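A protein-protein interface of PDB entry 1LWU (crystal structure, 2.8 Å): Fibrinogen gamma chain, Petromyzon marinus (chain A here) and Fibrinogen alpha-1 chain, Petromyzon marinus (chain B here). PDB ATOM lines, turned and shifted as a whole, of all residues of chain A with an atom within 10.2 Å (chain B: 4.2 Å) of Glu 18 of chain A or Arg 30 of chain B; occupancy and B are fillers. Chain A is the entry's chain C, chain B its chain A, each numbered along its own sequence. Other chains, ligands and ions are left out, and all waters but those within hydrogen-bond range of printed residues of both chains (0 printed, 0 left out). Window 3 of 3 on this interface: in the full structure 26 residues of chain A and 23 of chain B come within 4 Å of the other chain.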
ATOM      1  N   ILE A  10     -22.891  24.650  25.223  1.00  0.00           N
ATOM      2  CA  ILE A  10     -21.832  23.815  25.775  1.00  0.00           C
ATOM      3  C   ILE A  10     -20.847  23.481  24.663  1.00  0.00           C
ATOM      4  O   ILE A  10     -19.803  22.894  24.908  1.00  0.00           O
ATOM      5  CB  ILE A  10     -22.391  22.499  26.339  1.00  0.00           C
ATOM      6  CG1 ILE A  10     -23.489  22.802  27.358  1.00  0.00           C
ATOM      7  CG2 ILE A  10     -21.273  21.686  26.982  1.00  0.00           C
ATOM      8  CD1 ILE A  10     -24.249  21.575  27.822  1.00  0.00           C
ATOM      9  N   LEU A  11     -21.207  23.850  23.436  1.00  0.00           N
ATOM     10  CA  LEU A  11     -20.370  23.622  22.267  1.00  0.00           C
ATOM     11  C   LEU A  11     -19.549  24.871  22.015  1.00  0.00           C
ATOM     12  O   LEU A  11     -18.335  24.860  22.193  1.00  0.00           O
ATOM     13  CB  LEU A  11     -21.227  23.320  21.034  1.00  0.00           C
ATOM     14  CG  LEU A  11     -21.001  21.952  20.393  1.00  0.00           C
ATOM     15  CD1 LEU A  11     -21.468  20.864  21.340  1.00  0.00           C
ATOM     16  CD2 LEU A  11     -21.750  21.874  19.085  1.00  0.00           C
ATOM     17  N   GLU A  12     -20.216  25.945  21.596  1.00  0.00           N
ATOM     18  CA  GLU A  12     -19.531  27.207  21.338  1.00  0.00           C
ATOM     19  C   GLU A  12     -18.552  27.448  22.475  1.00  0.00           C
ATOM     20  O   GLU A  12     -17.420  27.880  22.252  1.00  0.00           O
ATOM     21  CB  GLU A  12     -20.526  28.362  21.276  1.00  0.00           C
ATOM     22  CG  GLU A  12     -21.445  28.330  20.081  1.00  0.00           C
ATOM     23  CD  GLU A  12     -22.516  29.400  20.155  1.00  0.00           C
ATOM     24  OE1 GLU A  12     -23.267  29.568  19.170  1.00  0.00           O
ATOM     25  OE2 GLU A  12     -22.608  30.072  21.205  1.00  0.00           O
ATOM     26  N   GLU A  13     -18.990  27.164  23.697  1.00  0.00           N
ATOM     27  CA  GLU A  13     -18.125  27.344  24.850  1.00  0.00           C
ATOM     28  C   GLU A  13     -16.841  26.562  24.614  1.00  0.00           C
ATOM     29  O   GLU A  13     -15.745  27.098  24.783  1.00  0.00           O
ATOM     30  CB  GLU A  13     -18.807  26.843  26.126  1.00  0.00           C
ATOM     31  CG  GLU A  13     -20.006  27.673  26.573  1.00  0.00           C
ATOM     32  CD  GLU A  13     -19.638  29.088  26.992  1.00  0.00           C
ATOM     33  OE1 GLU A  13     -19.133  29.860  26.145  1.00  0.00           O
ATOM     34  OE2 GLU A  13     -19.862  29.429  28.172  1.00  0.00           O
ATOM     35  N   VAL A  14     -16.977  25.304  24.203  1.00  0.00           N
ATOM     36  CA  VAL A  14     -15.810  24.462  23.954  1.00  0.00           C
ATOM     37  C   VAL A  14     -15.023  24.900  22.733  1.00  0.00           C
ATOM     38  O   VAL A  14     -13.816  24.726  22.682  1.00  0.00           O
ATOM     39  CB  VAL A  14     -16.201  22.991  23.797  1.00  0.00           C
ATOM     40  CG1 VAL A  14     -14.971  22.146  23.582  1.00  0.00           C
ATOM     41  CG2 VAL A  14     -16.911  22.521  25.045  1.00  0.00           C
ATOM     42  N   ARG A  15     -15.700  25.467  21.745  1.00  0.00           N
ATOM     43  CA  ARG A  15     -15.006  25.950  20.559  1.00  0.00           C
ATOM     44  C   ARG A  15     -14.081  27.076  21.010  1.00  0.00           C
ATOM     45  O   ARG A  15     -13.001  27.276  20.454  1.00  0.00           O
ATOM     46  CB  ARG A  15     -16.001  26.487  19.524  1.00  0.00           C
ATOM     47  CG  ARG A  15     -15.334  27.172  18.340  1.00  0.00           C
ATOM     48  CD  ARG A  15     -16.316  27.495  17.230  1.00  0.00           C
ATOM     49  NE  ARG A  15     -15.640  28.129  16.103  1.00  0.00           N
ATOM     50  CZ  ARG A  15     -16.211  28.388  14.932  1.00  0.00           C
ATOM     51  NH1 ARG A  15     -17.481  28.062  14.721  1.00  0.00           N
ATOM     52  NH2 ARG A  15     -15.513  28.979  13.971  1.00  0.00           N
ATOM     53  N   ILE A  16     -14.529  27.803  22.031  1.00  0.00           N
ATOM     54  CA  ILE A  16     -13.782  28.919  22.598  1.00  0.00           C
ATOM     55  C   ILE A  16     -12.654  28.427  23.504  1.00  0.00           C
ATOM     56  O   ILE A  16     -11.514  28.879  23.383  1.00  0.00           O
ATOM     57  CB  ILE A  16     -14.706  29.841  23.424  1.00  0.00           C
ATOM     58  CG1 ILE A  16     -15.754  30.484  22.511  1.00  0.00           C
ATOM     59  CG2 ILE A  16     -13.880  30.892  24.148  1.00  0.00           C
ATOM     60  CD1 ILE A  16     -15.175  31.356  21.409  1.00  0.00           C
ATOM     61  N   LEU A  17     -12.979  27.507  24.412  1.00  0.00           N
ATOM     62  CA  LEU A  17     -11.987  26.963  25.329  1.00  0.00           C
ATOM     63  C   LEU A  17     -10.824  26.313  24.591  1.00  0.00           C
ATOM     64  O   LEU A  17      -9.724  26.186  25.131  1.00  0.00           O
ATOM     65  CB  LEU A  17     -12.619  25.936  26.272  1.00  0.00           C
ATOM     66  CG  LEU A  17     -13.442  26.426  27.465  1.00  0.00           C
ATOM     67  CD1 LEU A  17     -13.641  25.260  28.440  1.00  0.00           C
ATOM     68  CD2 LEU A  17     -12.719  27.569  28.169  1.00  0.00           C
ATOM     69  N   GLU A  18     -11.069  25.882  23.362  1.00  0.00           N
ATOM     70  CA  GLU A  18     -10.017  25.267  22.576  1.00  0.00           C
ATOM     71  C   GLU A  18      -9.138  26.387  22.026  1.00  0.00           C
ATOM     72  O   GLU A  18      -7.915  26.335  22.130  1.00  0.00           O
ATOM     73  CB  GLU A  18     -10.625  24.433  21.445  1.00  0.00           C
ATOM     74  CG  GLU A  18     -11.412  23.213  21.941  1.00  0.00           C
ATOM     75  CD  GLU A  18     -11.928  22.310  20.817  1.00  0.00           C
ATOM     76  OE1 GLU A  18     -12.747  22.775  19.989  1.00  0.00           O
ATOM     77  OE2 GLU A  18     -11.513  21.128  20.770  1.00  0.00           O
ATOM     78  N   GLN A  19      -9.768  27.412  21.465  1.00  0.00           N
ATOM     79  CA  GLN A  19      -9.039  28.546  20.911  1.00  0.00           C
ATOM     80  C   GLN A  19      -8.116  29.151  21.960  1.00  0.00           C
ATOM     81  O   GLN A  19      -6.969  29.492  21.670  1.00  0.00           O
ATOM     82  CB  GLN A  19     -10.016  29.611  20.419  1.00  0.00           C
ATOM     83  CG  GLN A  19     -10.973  29.123  19.345  1.00  0.00           C
ATOM     84  CD  GLN A  19     -12.021  30.163  18.988  1.00  0.00           C
ATOM     85  OE1 GLN A  19     -11.719  31.187  18.365  1.00  0.00           O
ATOM     86  NE2 GLN A  19     -13.264  29.909  19.395  1.00  0.00           N
ATOM     87  N   ILE A  20      -8.623  29.289  23.179  1.00  0.00           N
ATOM     88  CA  ILE A  20      -7.833  29.846  24.268  1.00  0.00           C
ATOM     89  C   ILE A  20      -6.641  28.942  24.567  1.00  0.00           C
ATOM     90  O   ILE A  20      -5.508  29.367  24.412  1.00  0.00           O
ATOM     91  CB  ILE A  20      -8.678  30.007  25.551  1.00  0.00           C
ATOM     92  CG1 ILE A  20      -9.838  30.962  25.294  1.00  0.00           C
ATOM     93  CG2 ILE A  20      -7.823  30.550  26.674  1.00  0.00           C
ATOM     94  CD1 ILE A  20      -9.397  32.290  24.752  1.00  0.00           C
ATOM     95  N   GLY A  21      -6.913  27.704  24.987  1.00  0.00           N
ATOM     96  CA  GLY A  21      -5.865  26.742  25.306  1.00  0.00           C
ATOM     97  C   GLY A  21      -4.687  26.819  24.352  1.00  0.00           C
ATOM     98  O   GLY A  21      -3.525  26.889  24.774  1.00  0.00           O
ATOM     99  N   VAL A  22      -4.990  26.814  23.057  1.00  0.00           N
ATOM    100  CA  VAL A  22      -3.969  26.905  22.024  1.00  0.00           C
ATOM    101  C   VAL A  22      -3.136  28.169  22.227  1.00  0.00           C
ATOM    102  O   VAL A  22      -1.910  28.115  22.178  1.00  0.00           O
ATOM    103  CB  VAL A  22      -4.602  26.911  20.616  1.00  0.00           C
ATOM    104  CG1 VAL A  22      -3.561  27.268  19.569  1.00  0.00           C
ATOM    105  CG2 VAL A  22      -5.194  25.534  20.313  1.00  0.00           C
ATOM    106  N   SER A  23      -3.789  29.306  22.452  1.00  0.00           N
ATOM    107  CA  SER A  23      -3.047  30.544  22.691  1.00  0.00           C
ATOM    108  C   SER A  23      -2.211  30.386  23.961  1.00  0.00           C
ATOM    109  O   SER A  23      -1.089  30.881  24.056  1.00  0.00           O
ATOM    110  CB  SER A  23      -4.003  31.720  22.841  1.00  0.00           C
ATOM    111  OG  SER A  23      -4.657  31.969  21.616  1.00  0.00           O
ATOM    112  N   HIS A  24      -2.762  29.690  24.945  1.00  0.00           N
ATOM    113  CA  HIS A  24      -2.030  29.466  26.168  1.00  0.00           C
ATOM    114  C   HIS A  24      -0.787  28.661  25.849  1.00  0.00           C
ATOM    115  O   HIS A  24       0.248  28.836  26.490  1.00  0.00           O
ATOM    116  CB  HIS A  24      -2.901  28.740  27.174  1.00  0.00           C
ATOM    117  CG  HIS A  24      -3.848  29.646  27.890  1.00  0.00           C
ATOM    118  ND1 HIS A  24      -4.704  29.204  28.875  1.00  0.00           N
ATOM    119  CD2 HIS A  24      -4.046  30.982  27.787  1.00  0.00           C
ATOM    120  CE1 HIS A  24      -5.388  30.231  29.349  1.00  0.00           C
ATOM    121  NE2 HIS A  24      -5.007  31.321  28.706  1.00  0.00           N
ATOM    122  N   ASP A  25      -0.884  27.787  24.850  1.00  0.00           N
ATOM    123  CA  ASP A  25       0.262  26.982  24.437  1.00  0.00           C
ATOM    124  C   ASP A  25       1.301  27.875  23.745  1.00  0.00           C
ATOM    125  O   ASP A  25       2.485  27.530  23.675  1.00  0.00           O
ATOM    126  CB  ASP A  25      -0.166  25.865  23.483  1.00  0.00           C
ATOM    127  CG  ASP A  25      -0.974  24.782  24.173  1.00  0.00           C
ATOM    128  OD1 ASP A  25      -0.535  24.313  25.245  1.00  0.00           O
ATOM    129  OD2 ASP A  25      -2.038  24.393  23.637  1.00  0.00           O
ATOM    130  N   ALA A  26       0.856  29.020  23.235  1.00  0.00           N
ATOM    131  CA  ALA A  26       1.758  29.953  22.569  1.00  0.00           C
ATOM    132  C   ALA A  26       2.376  30.838  23.624  1.00  0.00           C
ATOM    133  O   ALA A  26       3.594  31.058  23.643  1.00  0.00           O
ATOM    134  CB  ALA A  26       1.006  30.813  21.579  1.00  0.00           C
ATOM    135  N   GLU B  26     -18.861  13.118  21.366  1.00  0.00           N
ATOM    136  CA  GLU B  26     -17.912  13.765  20.476  1.00  0.00           C
ATOM    137  C   GLU B  26     -17.552  15.105  21.106  1.00  0.00           C
ATOM    138  O   GLU B  26     -16.657  15.812  20.642  1.00  0.00           O
ATOM    139  CB  GLU B  26     -18.528  13.971  19.092  1.00  0.00           C
ATOM    140  CG  GLU B  26     -17.666  14.791  18.149  1.00  0.00           C
ATOM    141  CD  GLU B  26     -16.267  14.235  17.966  1.00  0.00           C
ATOM    142  OE1 GLU B  26     -15.432  14.942  17.359  1.00  0.00           O
ATOM    143  OE2 GLU B  26     -16.007  13.098  18.419  1.00  0.00           O
ATOM    144  N   LEU B  27     -18.275  15.457  22.163  1.00  0.00           N
ATOM    145  CA  LEU B  27     -18.001  16.686  22.887  1.00  0.00           C
ATOM    146  C   LEU B  27     -16.929  16.323  23.898  1.00  0.00           C
ATOM    147  O   LEU B  27     -15.938  17.036  24.052  1.00  0.00           O
ATOM    148  CB  LEU B  27     -19.241  17.188  23.629  1.00  0.00           C
ATOM    149  CG  LEU B  27     -19.886  18.470  23.104  1.00  0.00           C
ATOM    150  CD1 LEU B  27     -20.755  19.071  24.197  1.00  0.00           C
ATOM    151  CD2 LEU B  27     -18.814  19.464  22.693  1.00  0.00           C
ATOM    152  N   GLU B  28     -17.133  15.200  24.580  1.00  0.00           N
ATOM    153  CA  GLU B  28     -16.180  14.725  25.572  1.00  0.00           C
ATOM    154  C   GLU B  28     -14.851  14.394  24.915  1.00  0.00           C
ATOM    155  O   GLU B  28     -13.791  14.674  25.464  1.00  0.00           O
ATOM    156  CB  GLU B  28     -16.719  13.488  26.276  1.00  0.00           C
ATOM    157  CG  GLU B  28     -17.917  13.764  27.140  1.00  0.00           C
ATOM    158  CD  GLU B  28     -18.381  12.526  27.855  1.00  0.00           C
ATOM    159  OE1 GLU B  28     -19.358  12.617  28.626  1.00  0.00           O
ATOM    160  OE2 GLU B  28     -17.762  11.458  27.643  1.00  0.00           O
ATOM    161  N   ARG B  29     -14.904  13.794  23.733  1.00  0.00           N
ATOM    162  CA  ARG B  29     -13.674  13.466  23.031  1.00  0.00           C
ATOM    163  C   ARG B  29     -12.973  14.771  22.664  1.00  0.00           C
ATOM    164  O   ARG B  29     -11.825  14.774  22.215  1.00  0.00           O
ATOM    165  CB  ARG B  29     -13.980  12.638  21.773  1.00  0.00           C
ATOM    166  CG  ARG B  29     -13.698  13.321  20.438  1.00  0.00           C
ATOM    167  CD  ARG B  29     -13.240  12.289  19.428  1.00  0.00           C
ATOM    168  NE  ARG B  29     -12.036  11.614  19.908  1.00  0.00           N
ATOM    169  CZ  ARG B  29     -11.475  10.563  19.321  1.00  0.00           C
ATOM    170  NH1 ARG B  29     -12.009  10.057  18.218  1.00  0.00           N
ATOM    171  NH2 ARG B  29     -10.377  10.019  19.839  1.00  0.00           N
ATOM    172  N   ARG B  30     -13.680  15.882  22.864  1.00  0.00           N
ATOM    173  CA  ARG B  30     -13.149  17.202  22.567  1.00  0.00           C
ATOM    174  C   ARG B  30     -12.866  17.985  23.853  1.00  0.00           C
ATOM    175  O   ARG B  30     -11.996  18.858  23.887  1.00  0.00           O
ATOM    176  CB  ARG B  30     -14.126  17.980  21.679  1.00  0.00           C
ATOM    177  CG  ARG B  30     -13.603  19.352  21.289  1.00  0.00           C
ATOM    178  CD  ARG B  30     -14.445  20.036  20.230  1.00  0.00           C
ATOM    179  NE  ARG B  30     -14.483  19.280  18.983  1.00  0.00           N
ATOM    180  CZ  ARG B  30     -14.867  19.788  17.816  1.00  0.00           C
ATOM    181  NH1 ARG B  30     -15.238  21.059  17.738  1.00  0.00           N
ATOM    182  NH2 ARG B  30     -14.890  19.021  16.733  1.00  0.00           N
ATOM    183  N   ILE B  31     -13.604  17.666  24.910  1.00  0.00           N
ATOM    184  CA  ILE B  31     -13.422  18.329  26.189  1.00  0.00           C
ATOM    185  C   ILE B  31     -12.401  17.584  27.025  1.00  0.00           C
ATOM    186  O   ILE B  31     -11.567  18.197  27.682  1.00  0.00           O
ATOM    187  CB  ILE B  31     -14.754  18.423  26.966  1.00  0.00           C
ATOM    188  CG1 ILE B  31     -15.621  19.533  26.352  1.00  0.00           C
ATOM    189  CG2 ILE B  31     -14.490  18.674  28.458  1.00  0.00           C
ATOM    190  CD1 ILE B  31     -16.913  19.816  27.110  1.00  0.00           C
ATOM    191  N   ILE B  32     -12.463  16.258  26.993  1.00  0.00           N
ATOM    192  CA  ILE B  32     -11.521  15.448  27.755  1.00  0.00           C
ATOM    193  C   ILE B  32     -10.113  15.660  27.212  1.00  0.00           C
ATOM    194  O   ILE B  32      -9.129  15.293  27.851  1.00  0.00           O
ATOM    195  CB  ILE B  32     -11.861  13.940  27.680  1.00  0.00           C
ATOM    196  CG1 ILE B  32     -11.128  13.189  28.796  1.00  0.00           C
ATOM    197  CG2 ILE B  32     -11.449  13.372  26.315  1.00  0.00           C
ATOM    198  CD1 ILE B  32     -11.522  11.738  28.922  1.00  0.00           C
ATOM    199  N   HIS B  33     -10.012  16.236  26.020  1.00  0.00           N
ATOM    200  CA  HIS B  33      -8.697  16.503  25.470  1.00  0.00           C
ATOM    201  C   HIS B  33      -8.240  17.811  26.087  1.00  0.00           C
ATOM    202  O   HIS B  33      -7.079  17.945  26.480  1.00  0.00           O
ATOM    203  CB  HIS B  33      -8.725  16.645  23.955  1.00  0.00           C
ATOM    204  CG  HIS B  33      -7.360  16.766  23.353  1.00  0.00           C
ATOM    205  ND1 HIS B  33      -6.483  15.704  23.283  1.00  0.00           N
ATOM    206  CD2 HIS B  33      -6.691  17.840  22.869  1.00  0.00           C
ATOM    207  CE1 HIS B  33      -5.332  16.119  22.784  1.00  0.00           C
ATOM    208  NE2 HIS B  33      -5.431  17.411  22.525  1.00  0.00           N
ATOM    209  N   LEU B  34      -9.157  18.776  26.171  1.00  0.00           N
ATOM    210  CA  LEU B  34      -8.843  20.069  26.774  1.00  0.00           C
ATOM    211  C   LEU B  34      -8.157  19.799  28.110  1.00  0.00           C
ATOM    212  O   LEU B  34      -7.397  20.626  28.609  1.00  0.00           O
ATOM    213  CB  LEU B  34     -10.115  20.893  26.998  1.00  0.00           C
ATOM    214  CG  LEU B  34     -10.365  22.042  26.023  1.00  0.00           C
ATOM    215  CD1 LEU B  34     -11.692  22.686  26.323  1.00  0.00           C
ATOM    216  CD2 LEU B  34      -9.266  23.070  26.135  1.00  0.00           C
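NH1 of Arg 30 of chain B lies within salt-bridge range of OE1 of Glu 18 of chain A, 3.8 Å away.
CG2 of Ile 10 of chain A touches CD1 of Leu 27 of chain B (3.9 Å).
Leu 11 of chain A touches Leu 27 of chain B.
CG1 of Val 14 of chain A touches CG of Arg 30 of chain B, 3.9 Å away.
CG2 of Val 14 of chain A touches CD1 of Ile 31 of chain B (3.4 Å).
Leu 17 of chain A touches Leu 34 of chain B.
Arg 30 of chain B touches just these residues of chain A: Val 14 and Glu 18.
Of the printed residues of chain A, Leu 34 of chain B touches Leu 17.
Of the printed residues of chain B, Leu 17 of chain A touches Leu 34 (3.3 Å).
Of the printed residues of chain B, Leu 11 of chain A touches Leu 27.
His 33 of chain B touches none of the printed residues of chain A.
Glu 12 of chain A touches none of the printed residues of chain B.
The nearest residue of chain A that does not touch Arg 30 of chain B is Arg 15 of chain A (5.7 Å).
The nearest printed residue of chain B that does not touch Leu 11 of chain A is Arg 30 of chain B (6.4 Å).
Printed residues of chain B that touch a printed residue of chain A: Leu 27, Arg 30, Ile 31 and Leu 34.
Of the 17 printed residues of chain A, 5 touch a printed residue of chain B.
Hydrophobic or aromatic side chains of chain A that line the printed part of chain B: Ile 10, Leu 11, Val 14 and Leu 17.
Among the printed residues, 6 pairs touch across the chains.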
